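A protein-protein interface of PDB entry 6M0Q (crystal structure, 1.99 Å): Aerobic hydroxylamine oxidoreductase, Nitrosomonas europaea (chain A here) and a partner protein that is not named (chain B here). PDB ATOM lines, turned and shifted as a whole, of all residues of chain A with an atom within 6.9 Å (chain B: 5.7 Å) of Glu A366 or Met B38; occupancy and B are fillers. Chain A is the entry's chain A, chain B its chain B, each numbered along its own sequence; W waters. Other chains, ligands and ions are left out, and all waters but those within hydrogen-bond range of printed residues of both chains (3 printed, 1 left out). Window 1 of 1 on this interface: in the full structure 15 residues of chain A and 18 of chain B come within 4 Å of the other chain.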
ATOM      1  N   ASN A 218      39.151  20.098 -24.061  1.00  0.00           N
ATOM      2  CA  ASN A 218      38.656  18.894 -24.709  1.00  0.00           C
ATOM      3  C   ASN A 218      38.844  18.962 -26.214  1.00  0.00           C
ATOM      4  O   ASN A 218      38.140  18.272 -26.953  1.00  0.00           O
ATOM      5  CB  ASN A 218      37.188  18.678 -24.339  1.00  0.00           C
ATOM      6  CG  ASN A 218      36.957  18.893 -22.866  1.00  0.00           C
ATOM      7  OD1 ASN A 218      36.548  19.968 -22.449  1.00  0.00           O
ATOM      8  ND2 ASN A 218      37.303  17.897 -22.058  1.00  0.00           N
ATOM      9  N   GLN A 220      38.049  21.325 -28.181  1.00  0.00           N
ATOM     10  CA  GLN A 220      36.904  21.951 -28.840  1.00  0.00           C
ATOM     11  C   GLN A 220      37.292  22.582 -30.168  1.00  0.00           C
ATOM     12  O   GLN A 220      36.553  22.478 -31.157  1.00  0.00           O
ATOM     13  CB  GLN A 220      36.291  23.021 -27.936  1.00  0.00           C
ATOM     14  CG  GLN A 220      35.402  22.488 -26.811  1.00  0.00           C
ATOM     15  CD  GLN A 220      36.188  22.039 -25.572  1.00  0.00           C
ATOM     16  OE1 GLN A 220      37.421  21.968 -25.575  1.00  0.00           O
ATOM     17  NE2 GLN A 220      35.463  21.726 -24.505  1.00  0.00           N
ATOM     18  N   TRP A 355      33.960  31.326 -25.263  1.00  0.00           N
ATOM     19  CA  TRP A 355      32.938  30.911 -26.211  1.00  0.00           C
ATOM     20  C   TRP A 355      33.469  30.744 -27.620  1.00  0.00           C
ATOM     21  O   TRP A 355      32.928  29.931 -28.376  1.00  0.00           O
ATOM     22  CB  TRP A 355      31.808  31.944 -26.240  1.00  0.00           C
ATOM     23  CG  TRP A 355      30.853  31.772 -25.096  1.00  0.00           C
ATOM     24  CD1 TRP A 355      30.728  32.553 -23.967  1.00  0.00           C
ATOM     25  CD2 TRP A 355      29.852  30.755 -24.999  1.00  0.00           C
ATOM     26  NE1 TRP A 355      29.700  32.074 -23.186  1.00  0.00           N
ATOM     27  CE2 TRP A 355      29.164  30.958 -23.790  1.00  0.00           C
ATOM     28  CE3 TRP A 355      29.476  29.689 -25.829  1.00  0.00           C
ATOM     29  CZ2 TRP A 355      28.101  30.150 -23.396  1.00  0.00           C
ATOM     30  CZ3 TRP A 355      28.450  28.871 -25.422  1.00  0.00           C
ATOM     31  CH2 TRP A 355      27.768  29.109 -24.212  1.00  0.00           C
ATOM     32  N   PRO A 359      28.699  29.322 -30.572  1.00  0.00           N
ATOM     33  CA  PRO A 359      28.267  28.612 -29.356  1.00  0.00           C
ATOM     34  C   PRO A 359      27.966  27.153 -29.553  1.00  0.00           C
ATOM     35  O   PRO A 359      27.960  26.408 -28.567  1.00  0.00           O
ATOM     36  CB  PRO A 359      26.979  29.344 -28.970  1.00  0.00           C
ATOM     37  CG  PRO A 359      27.095  30.672 -29.601  1.00  0.00           C
ATOM     38  CD  PRO A 359      27.814  30.444 -30.902  1.00  0.00           C
ATOM     39  N   PHE A 360      27.669  26.729 -30.773  1.00  0.00           N
ATOM     40  CA  PHE A 360      27.213  25.377 -31.047  1.00  0.00           C
ATOM     41  C   PHE A 360      28.362  24.391 -31.259  1.00  0.00           C
ATOM     42  O   PHE A 360      28.109  23.186 -31.393  1.00  0.00           O
ATOM     43  CB  PHE A 360      26.313  25.393 -32.278  1.00  0.00           C
ATOM     44  CG  PHE A 360      26.988  25.990 -33.481  1.00  0.00           C
ATOM     45  CD1 PHE A 360      27.661  25.177 -34.390  1.00  0.00           C
ATOM     46  CD2 PHE A 360      27.018  27.371 -33.666  1.00  0.00           C
ATOM     47  CE1 PHE A 360      28.308  25.719 -35.486  1.00  0.00           C
ATOM     48  CE2 PHE A 360      27.678  27.926 -34.764  1.00  0.00           C
ATOM     49  CZ  PHE A 360      28.322  27.101 -35.673  1.00  0.00           C
ATOM     50  N   VAL A 361      29.603  24.867 -31.301  1.00  0.00           N
ATOM     51  CA  VAL A 361      30.729  23.946 -31.496  1.00  0.00           C
ATOM     52  C   VAL A 361      30.708  22.890 -30.400  1.00  0.00           C
ATOM     53  O   VAL A 361      30.622  23.246 -29.210  1.00  0.00           O
ATOM     54  CB  VAL A 361      32.057  24.713 -31.490  1.00  0.00           C
ATOM     55  CG1 VAL A 361      33.262  23.736 -31.348  1.00  0.00           C
ATOM     56  CG2 VAL A 361      32.174  25.532 -32.750  1.00  0.00           C
ATOM     57  N   PRO A 362      30.761  21.598 -30.735  1.00  0.00           N
ATOM     58  CA  PRO A 362      30.726  20.548 -29.704  1.00  0.00           C
ATOM     59  C   PRO A 362      31.697  20.811 -28.564  1.00  0.00           C
ATOM     60  O   PRO A 362      32.869  21.143 -28.777  1.00  0.00           O
ATOM     61  CB  PRO A 362      31.118  19.288 -30.482  1.00  0.00           C
ATOM     62  CG  PRO A 362      30.623  19.562 -31.867  1.00  0.00           C
ATOM     63  CD  PRO A 362      30.810  21.036 -32.094  1.00  0.00           C
ATOM     64  N   GLY A 363      31.189  20.675 -27.338  1.00  0.00           N
ATOM     65  CA  GLY A 363      31.978  20.813 -26.136  1.00  0.00           C
ATOM     66  C   GLY A 363      32.110  22.229 -25.620  1.00  0.00           C
ATOM     67  O   GLY A 363      32.524  22.410 -24.484  1.00  0.00           O
ATOM     68  N   ILE A 364      31.777  23.242 -26.427  1.00  0.00           N
ATOM     69  CA  ILE A 364      31.971  24.624 -25.997  1.00  0.00           C
ATOM     70  C   ILE A 364      30.934  25.006 -24.943  1.00  0.00           C
ATOM     71  O   ILE A 364      31.269  25.499 -23.860  1.00  0.00           O
ATOM     72  CB  ILE A 364      31.925  25.559 -27.220  1.00  0.00           C
ATOM     73  CG1 ILE A 364      33.186  25.378 -28.057  1.00  0.00           C
ATOM     74  CG2 ILE A 364      31.717  27.004 -26.808  1.00  0.00           C
ATOM     75  CD1 ILE A 364      34.435  25.951 -27.438  1.00  0.00           C
ATOM     76  N   ALA A 365      29.662  24.757 -25.224  1.00  0.00           N
ATOM     77  CA  ALA A 365      28.644  25.036 -24.220  1.00  0.00           C
ATOM     78  C   ALA A 365      28.890  24.226 -22.951  1.00  0.00           C
ATOM     79  O   ALA A 365      28.794  24.753 -21.838  1.00  0.00           O
ATOM     80  CB  ALA A 365      27.251  24.743 -24.785  1.00  0.00           C
ATOM     81  N   GLU A 366      29.201  22.934 -23.095  1.00  0.00           N
ATOM     82  CA  GLU A 366      29.389  22.091 -21.912  1.00  0.00           C
ATOM     83  C   GLU A 366      30.581  22.562 -21.087  1.00  0.00           C
ATOM     84  O   GLU A 366      30.580  22.454 -19.856  1.00  0.00           O
ATOM     85  CB  GLU A 366      29.586  20.626 -22.320  1.00  0.00           C
ATOM     86  CG  GLU A 366      28.395  19.957 -22.998  1.00  0.00           C
ATOM     87  CD  GLU A 366      28.322  20.211 -24.518  1.00  0.00           C
ATOM     88  OE1 GLU A 366      29.002  21.155 -25.021  1.00  0.00           O
ATOM     89  OE2 GLU A 366      27.576  19.459 -25.207  1.00  0.00           O
ATOM     90  N   ASN A 367      31.594  23.098 -21.748  1.00  0.00           N
ATOM     91  CA  ASN A 367      32.788  23.583 -21.090  1.00  0.00           C
ATOM     92  C   ASN A 367      32.599  24.934 -20.429  1.00  0.00           C
ATOM     93  O   ASN A 367      33.509  25.384 -19.728  1.00  0.00           O
ATOM     94  CB  ASN A 367      33.931  23.642 -22.119  1.00  0.00           C
ATOM     95  CG  ASN A 367      35.222  24.132 -21.527  1.00  0.00           C
ATOM     96  OD1 ASN A 367      35.717  23.564 -20.554  1.00  0.00           O
ATOM     97  ND2 ASN A 367      35.765  25.208 -22.090  1.00  0.00           N
ATOM     98  N   ILE A 368      31.437  25.581 -20.583  1.00  0.00           N
ATOM     99  CA  ILE A 368      31.338  26.956 -20.120  1.00  0.00           C
ATOM    100  C   ILE A 368      31.310  27.038 -18.599  1.00  0.00           C
ATOM    101  O   ILE A 368      31.623  28.088 -18.029  1.00  0.00           O
ATOM    102  CB  ILE A 368      30.125  27.650 -20.769  1.00  0.00           C
ATOM    103  CG1 ILE A 368      30.380  29.154 -20.897  1.00  0.00           C
ATOM    104  CG2 ILE A 368      28.832  27.350 -19.994  1.00  0.00           C
ATOM    105  CD1 ILE A 368      31.557  29.502 -21.816  1.00  0.00           C
ATOM    106  N   THR A 369      30.995  25.944 -17.912  1.00  0.00           N
ATOM    107  CA  THR A 369      30.983  25.934 -16.454  1.00  0.00           C
ATOM    108  C   THR A 369      32.253  25.349 -15.847  1.00  0.00           C
ATOM    109  O   THR A 369      32.348  25.251 -14.620  1.00  0.00           O
ATOM    110  CB  THR A 369      29.778  25.148 -15.940  1.00  0.00           C
ATOM    111  OG1 THR A 369      29.859  23.804 -16.429  1.00  0.00           O
ATOM    112  CG2 THR A 369      28.486  25.776 -16.440  1.00  0.00           C
ATOM    113  N   SER A 370      33.218  24.949 -16.668  1.00  0.00           N
ATOM    114  CA  SER A 370      34.398  24.279 -16.152  1.00  0.00           C
ATOM    115  C   SER A 370      35.276  25.257 -15.385  1.00  0.00           C
ATOM    116  O   SER A 370      35.157  26.479 -15.517  1.00  0.00           O
ATOM    117  CB  SER A 370      35.209  23.659 -17.292  1.00  0.00           C
ATOM    118  OG  SER A 370      35.816  24.684 -18.076  1.00  0.00           O
ATOM    119  N   SER A 373      37.095  27.487 -17.832  1.00  0.00           N
ATOM    120  CA  SER A 373      36.322  28.653 -18.277  1.00  0.00           C
ATOM    121  C   SER A 373      36.098  29.652 -17.150  1.00  0.00           C
ATOM    122  O   SER A 373      36.123  30.865 -17.386  1.00  0.00           O
ATOM    123  CB  SER A 373      34.965  28.233 -18.841  1.00  0.00           C
ATOM    124  OG  SER A 373      35.146  27.445 -19.996  1.00  0.00           O
ATOM    125  N   LEU A 405      23.317  30.468 -24.170  1.00  0.00           N
ATOM    126  CA  LEU A 405      22.729  29.137 -24.085  1.00  0.00           C
ATOM    127  C   LEU A 405      21.263  29.148 -24.517  1.00  0.00           C
ATOM    128  O   LEU A 405      20.779  28.177 -25.112  1.00  0.00           O
ATOM    129  CB  LEU A 405      22.878  28.614 -22.664  1.00  0.00           C
ATOM    130  CG  LEU A 405      24.291  28.308 -22.184  1.00  0.00           C
ATOM    131  CD1 LEU A 405      24.274  28.197 -20.663  1.00  0.00           C
ATOM    132  CD2 LEU A 405      24.743  26.997 -22.824  1.00  0.00           C
ATOM    133  N   LEU A 408      21.367  28.973 -28.055  1.00  0.00           N
ATOM    134  CA  LEU A 408      21.773  27.643 -28.481  1.00  0.00           C
ATOM    135  C   LEU A 408      20.623  26.649 -28.338  1.00  0.00           C
ATOM    136  O   LEU A 408      20.419  25.782 -29.205  1.00  0.00           O
ATOM    137  CB  LEU A 408      22.997  27.193 -27.687  1.00  0.00           C
ATOM    138  CG  LEU A 408      23.556  25.810 -28.029  1.00  0.00           C
ATOM    139  CD1 LEU A 408      23.978  25.718 -29.485  1.00  0.00           C
ATOM    140  CD2 LEU A 408      24.737  25.539 -27.112  1.00  0.00           C
ATOM    141  N   GLN A 412      19.163  24.325 -31.196  1.00  0.00           N
ATOM    142  CA  GLN A 412      19.223  22.873 -31.068  1.00  0.00           C
ATOM    143  C   GLN A 412      17.862  22.235 -31.318  1.00  0.00           C
ATOM    144  O   GLN A 412      17.772  21.156 -31.922  1.00  0.00           O
ATOM    145  CB  GLN A 412      19.766  22.507 -29.691  1.00  0.00           C
ATOM    146  CG  GLN A 412      21.281  22.686 -29.664  1.00  0.00           C
ATOM    147  CD  GLN A 412      21.866  22.446 -28.292  1.00  0.00           C
ATOM    148  OE1 GLN A 412      21.139  22.380 -27.293  1.00  0.00           O
ATOM    149  NE2 GLN A 412      23.188  22.333 -28.229  1.00  0.00           N
ATOM    150  N   LEU B  30      33.960  15.934 -24.278  1.00  0.00           N
ATOM    151  CA  LEU B  30      32.904  15.993 -23.279  1.00  0.00           C
ATOM    152  C   LEU B  30      31.642  15.309 -23.795  1.00  0.00           C
ATOM    153  O   LEU B  30      31.232  15.513 -24.948  1.00  0.00           O
ATOM    154  CB  LEU B  30      32.591  17.450 -22.951  1.00  0.00           C
ATOM    155  CG  LEU B  30      33.011  18.120 -21.650  1.00  0.00           C
ATOM    156  CD1 LEU B  30      34.099  17.353 -20.900  1.00  0.00           C
ATOM    157  CD2 LEU B  30      33.405  19.556 -21.972  1.00  0.00           C
ATOM    158  N   ALA B  31      31.020  14.508 -22.938  1.00  0.00           N
ATOM    159  CA  ALA B  31      29.711  13.964 -23.269  1.00  0.00           C
ATOM    160  C   ALA B  31      28.750  15.128 -23.507  1.00  0.00           C
ATOM    161  O   ALA B  31      28.745  16.091 -22.727  1.00  0.00           O
ATOM    162  CB  ALA B  31      29.197  13.051 -22.156  1.00  0.00           C
ATOM    163  N   PRO B  32      27.982  15.116 -24.587  1.00  0.00           N
ATOM    164  CA  PRO B  32      27.178  16.293 -24.904  1.00  0.00           C
ATOM    165  C   PRO B  32      26.100  16.520 -23.858  1.00  0.00           C
ATOM    166  O   PRO B  32      25.582  15.582 -23.244  1.00  0.00           O
ATOM    167  CB  PRO B  32      26.583  15.962 -26.277  1.00  0.00           C
ATOM    168  CG  PRO B  32      27.553  14.999 -26.865  1.00  0.00           C
ATOM    169  CD  PRO B  32      27.965  14.141 -25.688  1.00  0.00           C
ATOM    170  N   ILE B  33      25.824  17.792 -23.613  1.00  0.00           N
ATOM    171  CA  ILE B  33      24.722  18.217 -22.770  1.00  0.00           C
ATOM    172  C   ILE B  33      24.040  19.336 -23.531  1.00  0.00           C
ATOM    173  O   ILE B  33      24.701  20.286 -23.968  1.00  0.00           O
ATOM    174  CB  ILE B  33      25.181  18.690 -21.375  1.00  0.00           C
ATOM    175  CG1 ILE B  33      26.024  17.609 -20.684  1.00  0.00           C
ATOM    176  CG2 ILE B  33      23.964  19.116 -20.517  1.00  0.00           C
ATOM    177  CD1 ILE B  33      26.569  18.011 -19.327  1.00  0.00           C
ATOM    178  N   SER B  34      22.738  19.191 -23.738  1.00  0.00           N
ATOM    179  CA  SER B  34      21.980  20.179 -24.471  1.00  0.00           C
ATOM    180  C   SER B  34      22.027  21.522 -23.753  1.00  0.00           C
ATOM    181  O   SER B  34      22.260  21.615 -22.539  1.00  0.00           O
ATOM    182  CB  SER B  34      20.529  19.740 -24.606  1.00  0.00           C
ATOM    183  OG  SER B  34      19.923  19.822 -23.329  1.00  0.00           O
ATOM    184  N   ALA B  35      21.763  22.570 -24.524  1.00  0.00           N
ATOM    185  CA  ALA B  35      21.767  23.905 -23.954  1.00  0.00           C
ATOM    186  C   ALA B  35      20.684  24.052 -22.897  1.00  0.00           C
ATOM    187  O   ALA B  35      20.914  24.686 -21.857  1.00  0.00           O
ATOM    188  CB  ALA B  35      21.591  24.947 -25.061  1.00  0.00           C
ATOM    189  N   LYS B  36      19.491  23.481 -23.136  1.00  0.00           N
ATOM    190  CA  LYS B  36      18.427  23.636 -22.142  1.00  0.00           C
ATOM    191  C   LYS B  36      18.805  22.963 -20.834  1.00  0.00           C
ATOM    192  O   LYS B  36      18.439  23.445 -19.751  1.00  0.00           O
ATOM    193  CB  LYS B  36      17.107  23.077 -22.660  1.00  0.00           C
ATOM    194  CG  LYS B  36      17.136  21.608 -23.007  1.00  0.00           C
ATOM    195  CD  LYS B  36      15.775  21.174 -23.476  1.00  0.00           C
ATOM    196  CE  LYS B  36      14.804  21.150 -22.327  1.00  0.00           C
ATOM    197  NZ  LYS B  36      15.160  20.055 -21.391  1.00  0.00           N
ATOM    198  N   ASP B  37      19.545  21.858 -20.913  1.00  0.00           N
ATOM    199  CA  ASP B  37      19.974  21.178 -19.695  1.00  0.00           C
ATOM    200  C   ASP B  37      21.072  21.961 -18.985  1.00  0.00           C
ATOM    201  O   ASP B  37      21.085  22.027 -17.751  1.00  0.00           O
ATOM    202  CB  ASP B  37      20.439  19.752 -20.001  1.00  0.00           C
ATOM    203  CG  ASP B  37      19.282  18.793 -20.312  1.00  0.00           C
ATOM    204  OD1 ASP B  37      19.554  17.737 -20.934  1.00  0.00           O
ATOM    205  OD2 ASP B  37      18.115  19.079 -19.946  1.00  0.00           O
ATOM    206  N   MET B  38      22.004  22.551 -19.741  1.00  0.00           N
ATOM    207  CA  MET B  38      22.995  23.450 -19.149  1.00  0.00           C
ATOM    208  C   MET B  38      22.314  24.602 -18.428  1.00  0.00           C
ATOM    209  O   MET B  38      22.679  24.955 -17.295  1.00  0.00           O
ATOM    210  CB  MET B  38      23.932  23.990 -20.232  1.00  0.00           C
ATOM    211  CG  MET B  38      24.916  22.972 -20.792  1.00  0.00           C
ATOM    212  SD  MET B  38      25.994  22.287 -19.508  1.00  0.00           S
ATOM    213  CE  MET B  38      26.973  23.726 -19.024  1.00  0.00           C
ATOM    214  N   LEU B  39      21.316  25.203 -19.081  1.00  0.00           N
ATOM    215  CA  LEU B  39      20.560  26.277 -18.459  1.00  0.00           C
ATOM    216  C   LEU B  39      19.913  25.809 -17.166  1.00  0.00           C
ATOM    217  O   LEU B  39      20.044  26.462 -16.127  1.00  0.00           O
ATOM    218  CB  LEU B  39      19.514  26.804 -19.434  1.00  0.00           C
ATOM    219  CG  LEU B  39      20.230  27.725 -20.418  1.00  0.00           C
ATOM    220  CD1 LEU B  39      19.384  27.909 -21.641  1.00  0.00           C
ATOM    221  CD2 LEU B  39      20.565  29.055 -19.726  1.00  0.00           C
ATOM    222  N   ASP B  40      19.196  24.681 -17.218  1.00  0.00           N
ATOM    223  CA  ASP B  40      18.531  24.170 -16.022  1.00  0.00           C
ATOM    224  C   ASP B  40      19.540  23.845 -14.939  1.00  0.00           C
ATOM    225  O   ASP B  40      19.293  24.099 -13.756  1.00  0.00           O
ATOM    226  CB  ASP B  40      17.697  22.946 -16.386  1.00  0.00           C
ATOM    227  CG  ASP B  40      16.547  23.305 -17.338  1.00  0.00           C
ATOM    228  OD1 ASP B  40      16.330  24.527 -17.531  1.00  0.00           O
ATOM    229  OD2 ASP B  40      15.868  22.400 -17.874  1.00  0.00           O
ATOM    230  N   TYR B  41      20.693  23.307 -15.332  1.00  0.00           N
ATOM    231  CA  TYR B  41      21.749  23.002 -14.377  1.00  0.00           C
ATOM    232  C   TYR B  41      22.263  24.273 -13.698  1.00  0.00           C
ATOM    233  O   TYR B  41      22.368  24.333 -12.467  1.00  0.00           O
ATOM    234  CB  TYR B  41      22.862  22.250 -15.102  1.00  0.00           C
ATOM    235  CG  TYR B  41      23.930  21.735 -14.191  1.00  0.00           C
ATOM    236  CD1 TYR B  41      23.629  20.834 -13.173  1.00  0.00           C
ATOM    237  CD2 TYR B  41      25.241  22.137 -14.349  1.00  0.00           C
ATOM    238  CE1 TYR B  41      24.610  20.356 -12.330  1.00  0.00           C
ATOM    239  CE2 TYR B  41      26.227  21.661 -13.520  1.00  0.00           C
ATOM    240  CZ  TYR B  41      25.911  20.773 -12.519  1.00  0.00           C
ATOM    241  OH  TYR B  41      26.915  20.316 -11.706  1.00  0.00           O
ATOM    242  N   LEU B  42      22.528  25.325 -14.483  1.00  0.00           N
ATOM    243  CA  LEU B  42      22.924  26.602 -13.891  1.00  0.00           C
ATOM    244  C   LEU B  42      21.844  27.154 -12.970  1.00  0.00           C
ATOM    245  O   LEU B  42      22.146  27.714 -11.911  1.00  0.00           O
ATOM    246  CB  LEU B  42      23.232  27.619 -14.982  1.00  0.00           C
ATOM    247  CG  LEU B  42      24.443  27.291 -15.840  1.00  0.00           C
ATOM    248  CD1 LEU B  42      24.411  28.226 -17.007  1.00  0.00           C
ATOM    249  CD2 LEU B  42      25.716  27.467 -15.046  1.00  0.00           C
ATOM    250  N   ALA B  43      20.581  27.019 -13.366  1.00  0.00           N
ATOM    251  CA  ALA B  43      19.494  27.527 -12.549  1.00  0.00           C
ATOM    252  C   ALA B  43      19.406  26.777 -11.233  1.00  0.00           C
ATOM    253  O   ALA B  43      18.922  27.336 -10.249  1.00  0.00           O
ATOM    254  CB  ALA B  43      18.164  27.429 -13.309  1.00  0.00           C
ATOM    255  N   ILE B  72      17.762  17.405 -12.983  1.00  0.00           N
ATOM    256  CA  ILE B  72      18.779  17.951 -13.875  1.00  0.00           C
ATOM    257  C   ILE B  72      20.175  17.646 -13.340  1.00  0.00           C
ATOM    258  O   ILE B  72      21.086  17.308 -14.103  1.00  0.00           O
ATOM    259  CB  ILE B  72      18.559  19.462 -14.123  1.00  0.00           C
ATOM    260  CG1 ILE B  72      19.592  19.985 -15.123  1.00  0.00           C
ATOM    261  CG2 ILE B  72      18.637  20.267 -12.841  1.00  0.00           C
ATOM    262  CD1 ILE B  72      19.584  19.228 -16.417  1.00  0.00           C
ATOM    263  N   VAL B  76      23.069  15.727 -15.457  1.00  0.00           N
ATOM    264  CA  VAL B  76      24.388  16.260 -15.777  1.00  0.00           C
ATOM    265  C   VAL B  76      25.479  15.384 -15.182  1.00  0.00           C
ATOM    266  O   VAL B  76      26.487  15.104 -15.840  1.00  0.00           O
ATOM    267  CB  VAL B  76      24.515  17.719 -15.308  1.00  0.00           C
ATOM    268  CG1 VAL B  76      25.940  18.207 -15.483  1.00  0.00           C
ATOM    269  CG2 VAL B  76      23.570  18.588 -16.093  1.00  0.00           C
ATOM    270  N   ARG B  80      28.678  13.762 -16.873  1.00  0.00           N
ATOM    271  CA  ARG B  80      30.030  13.920 -16.343  1.00  0.00           C
ATOM    272  C   ARG B  80      30.687  12.573 -16.066  1.00  0.00           C
ATOM    273  O   ARG B  80      31.896  12.429 -16.272  1.00  0.00           O
ATOM    274  CB  ARG B  80      30.003  14.765 -15.067  1.00  0.00           C
ATOM    275  CG  ARG B  80      29.374  16.133 -15.229  1.00  0.00           C
ATOM    276  CD  ARG B  80      30.249  17.066 -16.030  1.00  0.00           C
ATOM    277  NE  ARG B  80      29.613  18.361 -16.302  1.00  0.00           N
ATOM    278  CZ  ARG B  80      29.463  19.323 -15.394  1.00  0.00           C
ATOM    279  NH1 ARG B  80      29.874  19.129 -14.139  1.00  0.00           N
ATOM    280  NH2 ARG B  80      28.898  20.475 -15.736  1.00  0.00           N
ATOM    281  N   TRP B  87      36.354  15.778 -18.154  1.00  0.00           N
ATOM    282  CA  TRP B  87      35.943  16.833 -17.228  1.00  0.00           C
ATOM    283  C   TRP B  87      37.002  16.974 -16.138  1.00  0.00           C
ATOM    284  O   TRP B  87      37.077  16.156 -15.218  1.00  0.00           O
ATOM    285  CB  TRP B  87      34.575  16.529 -16.635  1.00  0.00           C
ATOM    286  CG  TRP B  87      34.023  17.668 -15.837  1.00  0.00           C
ATOM    287  CD1 TRP B  87      33.944  17.759 -14.477  1.00  0.00           C
ATOM    288  CD2 TRP B  87      33.490  18.899 -16.354  1.00  0.00           C
ATOM    289  NE1 TRP B  87      33.373  18.963 -14.113  1.00  0.00           N
ATOM    290  CE2 TRP B  87      33.090  19.681 -15.246  1.00  0.00           C
ATOM    291  CE3 TRP B  87      33.304  19.410 -17.645  1.00  0.00           C
ATOM    292  CZ2 TRP B  87      32.510  20.946 -15.393  1.00  0.00           C
ATOM    293  CZ3 TRP B  87      32.729  20.664 -17.788  1.00  0.00           C
ATOM    294  CH2 TRP B  87      32.341  21.418 -16.667  1.00  0.00           C
HETATM  295  O   HOH W   1      18.810  22.497 -25.663  1.00  0.00           O
HETATM  296  O   HOH W   2      31.270  17.278 -26.880  1.00  0.00           O
HETATM  297  O   HOH W   3      24.724  22.006 -26.027  1.00  0.00           O
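OD1 of Asn A218 touches CD2 of Leu B30 (3.2 Å).
Gln A220 touches Leu B30 (NE2 to CD2, 3.9 Å).
O of Ala A365 touches CE of Met B38, at 3.5 Å.
Glu A366 touches Ala B31 (CG to O, 3.9 Å).
Glu A366 touches Pro B32.
O of Glu A366 touches CE of Met B38, 3.9 Å away.
CG2 of Thr A369 touches CE of Met B38, 3.6 Å away.
Ala B35 touches Leu A405.
Leu A405 touches Leu B39 (CB to CG, 3.6 Å).
OE1 of Gln A412 touches CA of Ser B34, 3.7 Å away.
The side-chain amide oxygen (OD1) of Asn A218 sits at hydrogen-bond distance from the side-chain amide nitrogen (NE2) of Gln A220 (2.9 Å).
The side-chain amide nitrogen (NE2) of Gln A220 lies within hydrogen-bond range of the backbone carbonyl oxygen (O) of Gly A363 (3.0 Å).
The side-chain carboxylate (OE1) of Glu A366 lies close to the backbone NH (N) of Gly A363, at 3.2 Å.
The backbone carbonyl oxygen (O) of Asn A367 is in hydrogen-bond range of the side-chain hydroxyl (OG) of Ser A373 (2.6 Å).
The backbone NH (N) of Ser A373 lies within hydrogen-bond range of the side-chain hydroxyl (OG) of Ser A370 (3.1 Å).
The side-chain hydroxyl (OG) of Ser B34 sits at hydrogen-bond distance from the backbone NH (N) of Asp B37 (3.2 Å).
Water W2 bridges O of Leu B30 (2.6 Å) and N of Gly A363 (3.4 Å).
Water W3 lies within hydrogen-bond range of O of Ile B33 (2.7 Å), NE2 of Gln A412 (2.7 Å) and N of Ala B35 (3.4 Å).
Water W1 lies within hydrogen-bond range of N of Lys B36 (2.8 Å), OE1 of Gln A412 (2.8 Å) and N of Ala B35 (3.2 Å).
Printed residues of chain B that touch a printed residue of chain A: Leu B30, Ala B31, Pro B32, Ile B33, Ser B34, Ala B35, Met B38, Leu B39, Leu B42, Arg B80 and Trp B87.
Hydrophobic or aromatic side chains of chain A within 4 Å of the printed part of chain B: Leu A405 and Leu A408.
Among the printed residues, 22 pairs touch across the chains.
Among the printed residues, no Asp or Glu carboxylate lies within 4 Å of a Lys or Arg side-chain nitrogen of the other chain.
OE2 of Glu A366 lies within hydrogen-bond range of N of Ile B33, 2.9 Å away.
OE1 of Gln A412 lies within hydrogen-bond range of N of Ala B35, at 2.8 Å.
Of the printed residues of chain B, Gln A220 touches Leu B30 (3.9 Å).
Phe A360 touches none of the printed residues of chain B.
Printed residues of chain B within 4 Å of Glu A366: Leu B30, Ala B31, Pro B32, Ile B33, Met B38 and Trp B87.
Printed residues of chain B within 4 Å of Leu A408: Ala B35 (3.7 Å).
Of the printed residues of chain A, Met B38 touches Ala A365, Glu A366 and Thr A369.
Printed residues of chain A within 4 Å of Trp B87: Glu A366, Thr A369 and Ser A370.
The nearest printed residue of chain B that does not touch Glu A366 is Arg B80 (4.9 Å).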
